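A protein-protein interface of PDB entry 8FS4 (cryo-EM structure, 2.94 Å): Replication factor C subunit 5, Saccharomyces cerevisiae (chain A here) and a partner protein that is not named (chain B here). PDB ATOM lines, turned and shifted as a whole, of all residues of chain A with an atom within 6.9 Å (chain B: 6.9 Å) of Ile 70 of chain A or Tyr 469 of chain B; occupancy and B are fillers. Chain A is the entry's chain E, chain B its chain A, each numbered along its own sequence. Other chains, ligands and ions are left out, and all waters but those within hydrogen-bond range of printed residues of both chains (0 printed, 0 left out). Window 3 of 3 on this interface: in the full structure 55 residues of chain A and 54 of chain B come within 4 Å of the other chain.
O of Ser 467 of chain B sits at hydrogen-bond distance from N of Asn 472 of chain B, 3.1 Å away.
OD1 of Asn 472 of chain B touches CB of Leu 68 of chain A, at 3.8 Å.
Tyr 469 of chain B touches Ile 70 of chain A (OH to CG2, 3.7 Å).
CG1 of Val 88 of chain A touches CD2 of Leu 468 of chain B, 3.6 Å away.
Of the printed residues of chain B, Leu 68 of chain A touches Asn 472 (3.8 Å).
Of the printed residues of chain B, Ile 70 of chain A touches Tyr 469 (3.7 Å).
Printed residues of chain B within 4 Å of Val 88 of chain A: Leu 468.
Leu 464 of chain B touches none of the printed residues of chain A.
Of the printed residues of chain A, Leu 468 of chain B touches Val 88.
Of chain A, only Ile 70 comes within 4 Å of Tyr 469 of chain B.
Of the printed residues of chain A, Asn 472 of chain B touches Leu 68 (3.8 Å).
The nearest residue of chain B that does not touch Ile 70 of chain A is Leu 468 of chain B (4.1 Å).
The nearest residue of chain A that does not touch Tyr 469 of chain B is Lys 69 of chain A (6.6 Å).
The nearest printed residue of chain B that does not touch Val 88 of chain A is Leu 464 of chain B (6.1 Å).
Hydrophobic or aromatic side chains of chain A within 4 Å of the printed part of chain B: Leu 68, Ile 70 and Val 88.
Along chain A the printed residues that touch a printed residue of chain B span positions 68 to 88.
Of the 10 printed residues of chain B, 3 touch a printed residue of chain A.
Among the printed residues, no Asp or Glu carboxylate lies within 4 Å of a Lys or Arg side-chain nitrogen of the other chain.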
ATOM      1  N   LEU A  68     -19.523 -15.043   1.818  1.00  0.00           N
ATOM      2  CA  LEU A  68     -20.055 -14.952   3.170  1.00  0.00           C
ATOM      3  C   LEU A  68     -19.076 -15.531   4.182  1.00  0.00           C
ATOM      4  O   LEU A  68     -18.402 -16.530   3.914  1.00  0.00           O
ATOM      5  CB  LEU A  68     -21.389 -15.692   3.270  1.00  0.00           C
ATOM      6  CG  LEU A  68     -22.434 -15.368   2.202  1.00  0.00           C
ATOM      7  CD1 LEU A  68     -23.748 -16.057   2.526  1.00  0.00           C
ATOM      8  CD2 LEU A  68     -22.634 -13.867   2.076  1.00  0.00           C
ATOM      9  N   LYS A  69     -19.005 -14.891   5.347  1.00  0.00           N
ATOM     10  CA  LYS A  69     -18.233 -15.398   6.470  1.00  0.00           C
ATOM     11  C   LYS A  69     -19.009 -15.133   7.751  1.00  0.00           C
ATOM     12  O   LYS A  69     -19.771 -14.167   7.844  1.00  0.00           O
ATOM     13  CB  LYS A  69     -16.841 -14.758   6.529  1.00  0.00           C
ATOM     14  CG  LYS A  69     -16.848 -13.230   6.479  1.00  0.00           C
ATOM     15  CD  LYS A  69     -15.728 -12.594   7.311  1.00  0.00           C
ATOM     16  CE  LYS A  69     -15.743 -13.040   8.769  1.00  0.00           C
ATOM     17  NZ  LYS A  69     -14.720 -12.348   9.597  1.00  0.00           N
ATOM     18  N   ILE A  70     -18.804 -15.997   8.741  1.00  0.00           N
ATOM     19  CA  ILE A  70     -19.646 -16.035   9.933  1.00  0.00           C
ATOM     20  C   ILE A  70     -18.982 -15.246  11.053  1.00  0.00           C
ATOM     21  O   ILE A  70     -17.784 -15.402  11.313  1.00  0.00           O
ATOM     22  CB  ILE A  70     -19.919 -17.487  10.366  1.00  0.00           C
ATOM     23  CG1 ILE A  70     -20.809 -17.535  11.613  1.00  0.00           C
ATOM     24  CG2 ILE A  70     -18.616 -18.227  10.650  1.00  0.00           C
ATOM     25  CD1 ILE A  70     -22.090 -16.741  11.513  1.00  0.00           C
ATOM     26  N   ASP A  71     -19.764 -14.395  11.716  1.00  0.00           N
ATOM     27  CA  ASP A  71     -19.311 -13.609  12.858  1.00  0.00           C
ATOM     28  C   ASP A  71     -20.151 -13.975  14.072  1.00  0.00           C
ATOM     29  O   ASP A  71     -21.385 -13.943  14.010  1.00  0.00           O
ATOM     30  CB  ASP A  71     -19.416 -12.110  12.570  1.00  0.00           C
ATOM     31  CG  ASP A  71     -18.416 -11.647  11.534  1.00  0.00           C
ATOM     32  OD1 ASP A  71     -17.484 -12.417  11.230  1.00  0.00           O
ATOM     33  OD2 ASP A  71     -18.565 -10.517  11.023  1.00  0.00           O
ATOM     34  N   VAL A  72     -19.484 -14.314  15.171  1.00  0.00           N
ATOM     35  CA  VAL A  72     -20.166 -14.632  16.421  1.00  0.00           C
ATOM     36  C   VAL A  72     -20.389 -13.333  17.187  1.00  0.00           C
ATOM     37  O   VAL A  72     -19.433 -12.647  17.561  1.00  0.00           O
ATOM     38  CB  VAL A  72     -19.353 -15.637  17.251  1.00  0.00           C
ATOM     39  CG1 VAL A  72     -20.076 -15.996  18.545  1.00  0.00           C
ATOM     40  CG2 VAL A  72     -19.074 -16.891  16.437  1.00  0.00           C
ATOM     41  N   GLU A  84     -26.115 -15.625  22.339  1.00  0.00           N
ATOM     42  CA  GLU A  84     -25.296 -15.700  21.138  1.00  0.00           C
ATOM     43  C   GLU A  84     -26.188 -15.712  19.904  1.00  0.00           C
ATOM     44  O   GLU A  84     -27.245 -16.350  19.896  1.00  0.00           O
ATOM     45  CB  GLU A  84     -24.409 -16.954  21.157  1.00  0.00           C
ATOM     46  CG  GLU A  84     -23.169 -16.870  20.275  1.00  0.00           C
ATOM     47  CD  GLU A  84     -23.496 -16.828  18.795  1.00  0.00           C
ATOM     48  OE1 GLU A  84     -24.285 -17.680  18.336  1.00  0.00           O
ATOM     49  OE2 GLU A  84     -22.981 -15.932  18.094  1.00  0.00           O
ATOM     50  N   LEU A  85     -25.754 -15.001  18.864  1.00  0.00           N
ATOM     51  CA  LEU A  85     -26.448 -14.978  17.584  1.00  0.00           C
ATOM     52  C   LEU A  85     -25.424 -15.087  16.466  1.00  0.00           C
ATOM     53  O   LEU A  85     -24.444 -14.336  16.446  1.00  0.00           O
ATOM     54  CB  LEU A  85     -27.273 -13.696  17.426  1.00  0.00           C
ATOM     55  CG  LEU A  85     -27.999 -13.488  16.094  1.00  0.00           C
ATOM     56  CD1 LEU A  85     -29.308 -14.255  16.070  1.00  0.00           C
ATOM     57  CD2 LEU A  85     -28.242 -12.009  15.860  1.00  0.00           C
ATOM     58  N   ASN A  86     -25.649 -16.019  15.544  1.00  0.00           N
ATOM     59  CA  ASN A  86     -24.788 -16.138  14.375  1.00  0.00           C
ATOM     60  C   ASN A  86     -25.064 -14.992  13.411  1.00  0.00           C
ATOM     61  O   ASN A  86     -26.220 -14.709  13.081  1.00  0.00           O
ATOM     62  CB  ASN A  86     -25.018 -17.480  13.683  1.00  0.00           C
ATOM     63  CG  ASN A  86     -24.532 -18.652  14.508  1.00  0.00           C
ATOM     64  OD1 ASN A  86     -23.992 -18.475  15.600  1.00  0.00           O
ATOM     65  ND2 ASN A  86     -24.722 -19.859  13.990  1.00  0.00           N
ATOM     66  N   VAL A  87     -24.002 -14.333  12.957  1.00  0.00           N
ATOM     67  CA  VAL A  87     -24.106 -13.195  12.051  1.00  0.00           C
ATOM     68  C   VAL A  87     -23.248 -13.514  10.834  1.00  0.00           C
ATOM     69  O   VAL A  87     -22.023 -13.348  10.865  1.00  0.00           O
ATOM     70  CB  VAL A  87     -23.666 -11.885  12.712  1.00  0.00           C
ATOM     71  CG1 VAL A  87     -23.734 -10.735  11.715  1.00  0.00           C
ATOM     72  CG2 VAL A  87     -24.525 -11.588  13.927  1.00  0.00           C
ATOM     73  N   VAL A  88     -23.882 -13.974   9.761  1.00  0.00           N
ATOM     74  CA  VAL A  88     -23.193 -14.160   8.489  1.00  0.00           C
ATOM     75  C   VAL A  88     -23.187 -12.820   7.765  1.00  0.00           C
ATOM     76  O   VAL A  88     -24.240 -12.207   7.560  1.00  0.00           O
ATOM     77  CB  VAL A  88     -23.858 -15.256   7.642  1.00  0.00           C
ATOM     78  CG1 VAL A  88     -23.750 -16.599   8.335  1.00  0.00           C
ATOM     79  CG2 VAL A  88     -25.308 -14.930   7.359  1.00  0.00           C
ATOM     80  N   SER A  89     -21.999 -12.354   7.392  1.00  0.00           N
ATOM     81  CA  SER A  89     -21.822 -11.010   6.866  1.00  0.00           C
ATOM     82  C   SER A  89     -21.079 -11.062   5.540  1.00  0.00           C
ATOM     83  O   SER A  89     -20.364 -12.020   5.238  1.00  0.00           O
ATOM     84  CB  SER A  89     -21.055 -10.123   7.853  1.00  0.00           C
ATOM     85  OG  SER A  89     -19.817 -10.713   8.208  1.00  0.00           O
ATOM     86  N   LEU B 464     -25.307 -26.876  10.361  1.00  0.00           N
ATOM     87  CA  LEU B 464     -25.245 -25.545   9.768  1.00  0.00           C
ATOM     88  C   LEU B 464     -23.807 -25.054   9.676  1.00  0.00           C
ATOM     89  O   LEU B 464     -23.372 -24.581   8.621  1.00  0.00           O
ATOM     90  CB  LEU B 464     -26.095 -24.551  10.558  1.00  0.00           C
ATOM     91  CG  LEU B 464     -26.518 -23.324   9.735  1.00  0.00           C
ATOM     92  CD1 LEU B 464     -27.565 -22.510  10.470  1.00  0.00           C
ATOM     93  CD2 LEU B 464     -25.331 -22.436   9.364  1.00  0.00           C
ATOM     94  N   ASN B 465     -23.047 -25.143  10.772  1.00  0.00           N
ATOM     95  CA  ASN B 465     -21.695 -24.587  10.725  1.00  0.00           C
ATOM     96  C   ASN B 465     -20.794 -25.400   9.800  1.00  0.00           C
ATOM     97  O   ASN B 465     -19.941 -24.835   9.103  1.00  0.00           O
ATOM     98  CB  ASN B 465     -21.085 -24.478  12.123  1.00  0.00           C
ATOM     99  CG  ASN B 465     -20.957 -25.808  12.821  1.00  0.00           C
ATOM    100  OD1 ASN B 465     -20.299 -26.726  12.331  1.00  0.00           O
ATOM    101  ND2 ASN B 465     -21.547 -25.902  14.004  1.00  0.00           N
ATOM    102  N   VAL B 466     -20.970 -26.725   9.764  1.00  0.00           N
ATOM    103  CA  VAL B 466     -20.220 -27.534   8.806  1.00  0.00           C
ATOM    104  C   VAL B 466     -20.477 -27.032   7.394  1.00  0.00           C
ATOM    105  O   VAL B 466     -19.547 -26.832   6.603  1.00  0.00           O
ATOM    106  CB  VAL B 466     -20.591 -29.022   8.938  1.00  0.00           C
ATOM    107  CG1 VAL B 466     -19.952 -29.828   7.810  1.00  0.00           C
ATOM    108  CG2 VAL B 466     -20.168 -29.562  10.291  1.00  0.00           C
ATOM    109  N   SER B 467     -21.749 -26.816   7.057  1.00  0.00           N
ATOM    110  CA  SER B 467     -22.078 -26.321   5.726  1.00  0.00           C
ATOM    111  C   SER B 467     -21.453 -24.955   5.484  1.00  0.00           C
ATOM    112  O   SER B 467     -20.929 -24.684   4.398  1.00  0.00           O
ATOM    113  CB  SER B 467     -23.593 -26.255   5.555  1.00  0.00           C
ATOM    114  OG  SER B 467     -24.184 -27.519   5.795  1.00  0.00           O
ATOM    115  N   LEU B 468     -21.489 -24.085   6.493  1.00  0.00           N
ATOM    116  CA  LEU B 468     -20.960 -22.736   6.347  1.00  0.00           C
ATOM    117  C   LEU B 468     -19.454 -22.713   6.140  1.00  0.00           C
ATOM    118  O   LEU B 468     -18.943 -21.778   5.516  1.00  0.00           O
ATOM    119  CB  LEU B 468     -21.319 -21.901   7.577  1.00  0.00           C
ATOM    120  CG  LEU B 468     -21.680 -20.422   7.424  1.00  0.00           C
ATOM    121  CD1 LEU B 468     -22.324 -20.105   6.095  1.00  0.00           C
ATOM    122  CD2 LEU B 468     -22.606 -20.027   8.567  1.00  0.00           C
ATOM    123  N   TYR B 469     -18.733 -23.707   6.656  1.00  0.00           N
ATOM    124  CA  TYR B 469     -17.288 -23.753   6.498  1.00  0.00           C
ATOM    125  C   TYR B 469     -16.826 -24.656   5.368  1.00  0.00           C
ATOM    126  O   TYR B 469     -15.674 -24.542   4.941  1.00  0.00           O
ATOM    127  CB  TYR B 469     -16.629 -24.230   7.801  1.00  0.00           C
ATOM    128  CG  TYR B 469     -16.356 -23.123   8.794  1.00  0.00           C
ATOM    129  CD1 TYR B 469     -15.963 -21.862   8.372  1.00  0.00           C
ATOM    130  CD2 TYR B 469     -16.483 -23.348  10.157  1.00  0.00           C
ATOM    131  CE1 TYR B 469     -15.716 -20.856   9.274  1.00  0.00           C
ATOM    132  CE2 TYR B 469     -16.237 -22.346  11.069  1.00  0.00           C
ATOM    133  CZ  TYR B 469     -15.852 -21.100  10.622  1.00  0.00           C
ATOM    134  OH  TYR B 469     -15.602 -20.093  11.523  1.00  0.00           O
ATOM    135  N   LYS B 470     -17.691 -25.535   4.876  1.00  0.00           N
ATOM    136  CA  LYS B 470     -17.325 -26.516   3.874  1.00  0.00           C
ATOM    137  C   LYS B 470     -18.093 -26.354   2.570  1.00  0.00           C
ATOM    138  O   LYS B 470     -17.682 -26.933   1.557  1.00  0.00           O
ATOM    139  CB  LYS B 470     -17.543 -27.927   4.446  1.00  0.00           C
ATOM    140  CG  LYS B 470     -17.027 -29.088   3.614  1.00  0.00           C
ATOM    141  CD  LYS B 470     -17.174 -30.386   4.406  1.00  0.00           C
ATOM    142  CE  LYS B 470     -16.795 -31.615   3.598  1.00  0.00           C
ATOM    143  NZ  LYS B 470     -17.031 -32.870   4.370  1.00  0.00           N
ATOM    144  N   TYR B 471     -19.195 -25.585   2.562  1.00  0.00           N
ATOM    145  CA  TYR B 471     -19.957 -25.391   1.332  1.00  0.00           C
ATOM    146  C   TYR B 471     -20.463 -23.958   1.159  1.00  0.00           C
ATOM    147  O   TYR B 471     -21.293 -23.723   0.273  1.00  0.00           O
ATOM    148  CB  TYR B 471     -21.178 -26.340   1.267  1.00  0.00           C
ATOM    149  CG  TYR B 471     -20.890 -27.785   1.626  1.00  0.00           C
ATOM    150  CD1 TYR B 471     -20.502 -28.145   2.907  1.00  0.00           C
ATOM    151  CD2 TYR B 471     -20.997 -28.788   0.676  1.00  0.00           C
ATOM    152  CE1 TYR B 471     -20.234 -29.455   3.233  1.00  0.00           C
ATOM    153  CE2 TYR B 471     -20.730 -30.107   0.994  1.00  0.00           C
ATOM    154  CZ  TYR B 471     -20.347 -30.433   2.277  1.00  0.00           C
ATOM    155  OH  TYR B 471     -20.077 -31.740   2.612  1.00  0.00           O
ATOM    156  N   ASN B 472     -19.989 -23.000   1.959  1.00  0.00           N
ATOM    157  CA  ASN B 472     -20.516 -21.637   1.942  1.00  0.00           C
ATOM    158  C   ASN B 472     -22.034 -21.691   1.825  1.00  0.00           C
ATOM    159  O   ASN B 472     -22.615 -21.150   0.878  1.00  0.00           O
ATOM    160  CB  ASN B 472     -19.902 -20.831   0.790  1.00  0.00           C
ATOM    161  CG  ASN B 472     -20.527 -19.450   0.632  1.00  0.00           C
ATOM    162  OD1 ASN B 472     -21.350 -19.028   1.444  1.00  0.00           O
ATOM    163  ND2 ASN B 472     -20.142 -18.745  -0.426  1.00  0.00           N
ATOM    164  N   ALA B 473     -22.685 -22.365   2.768  1.00  0.00           N
ATOM    165  CA  ALA B 473     -24.123 -22.591   2.721  1.00  0.00           C
ATOM    166  C   ALA B 473     -24.753 -22.131   4.026  1.00  0.00           C
ATOM    167  O   ALA B 473     -24.374 -22.604   5.102  1.00  0.00           O
ATOM    168  CB  ALA B 473     -24.424 -24.068   2.464  1.00  0.00           C
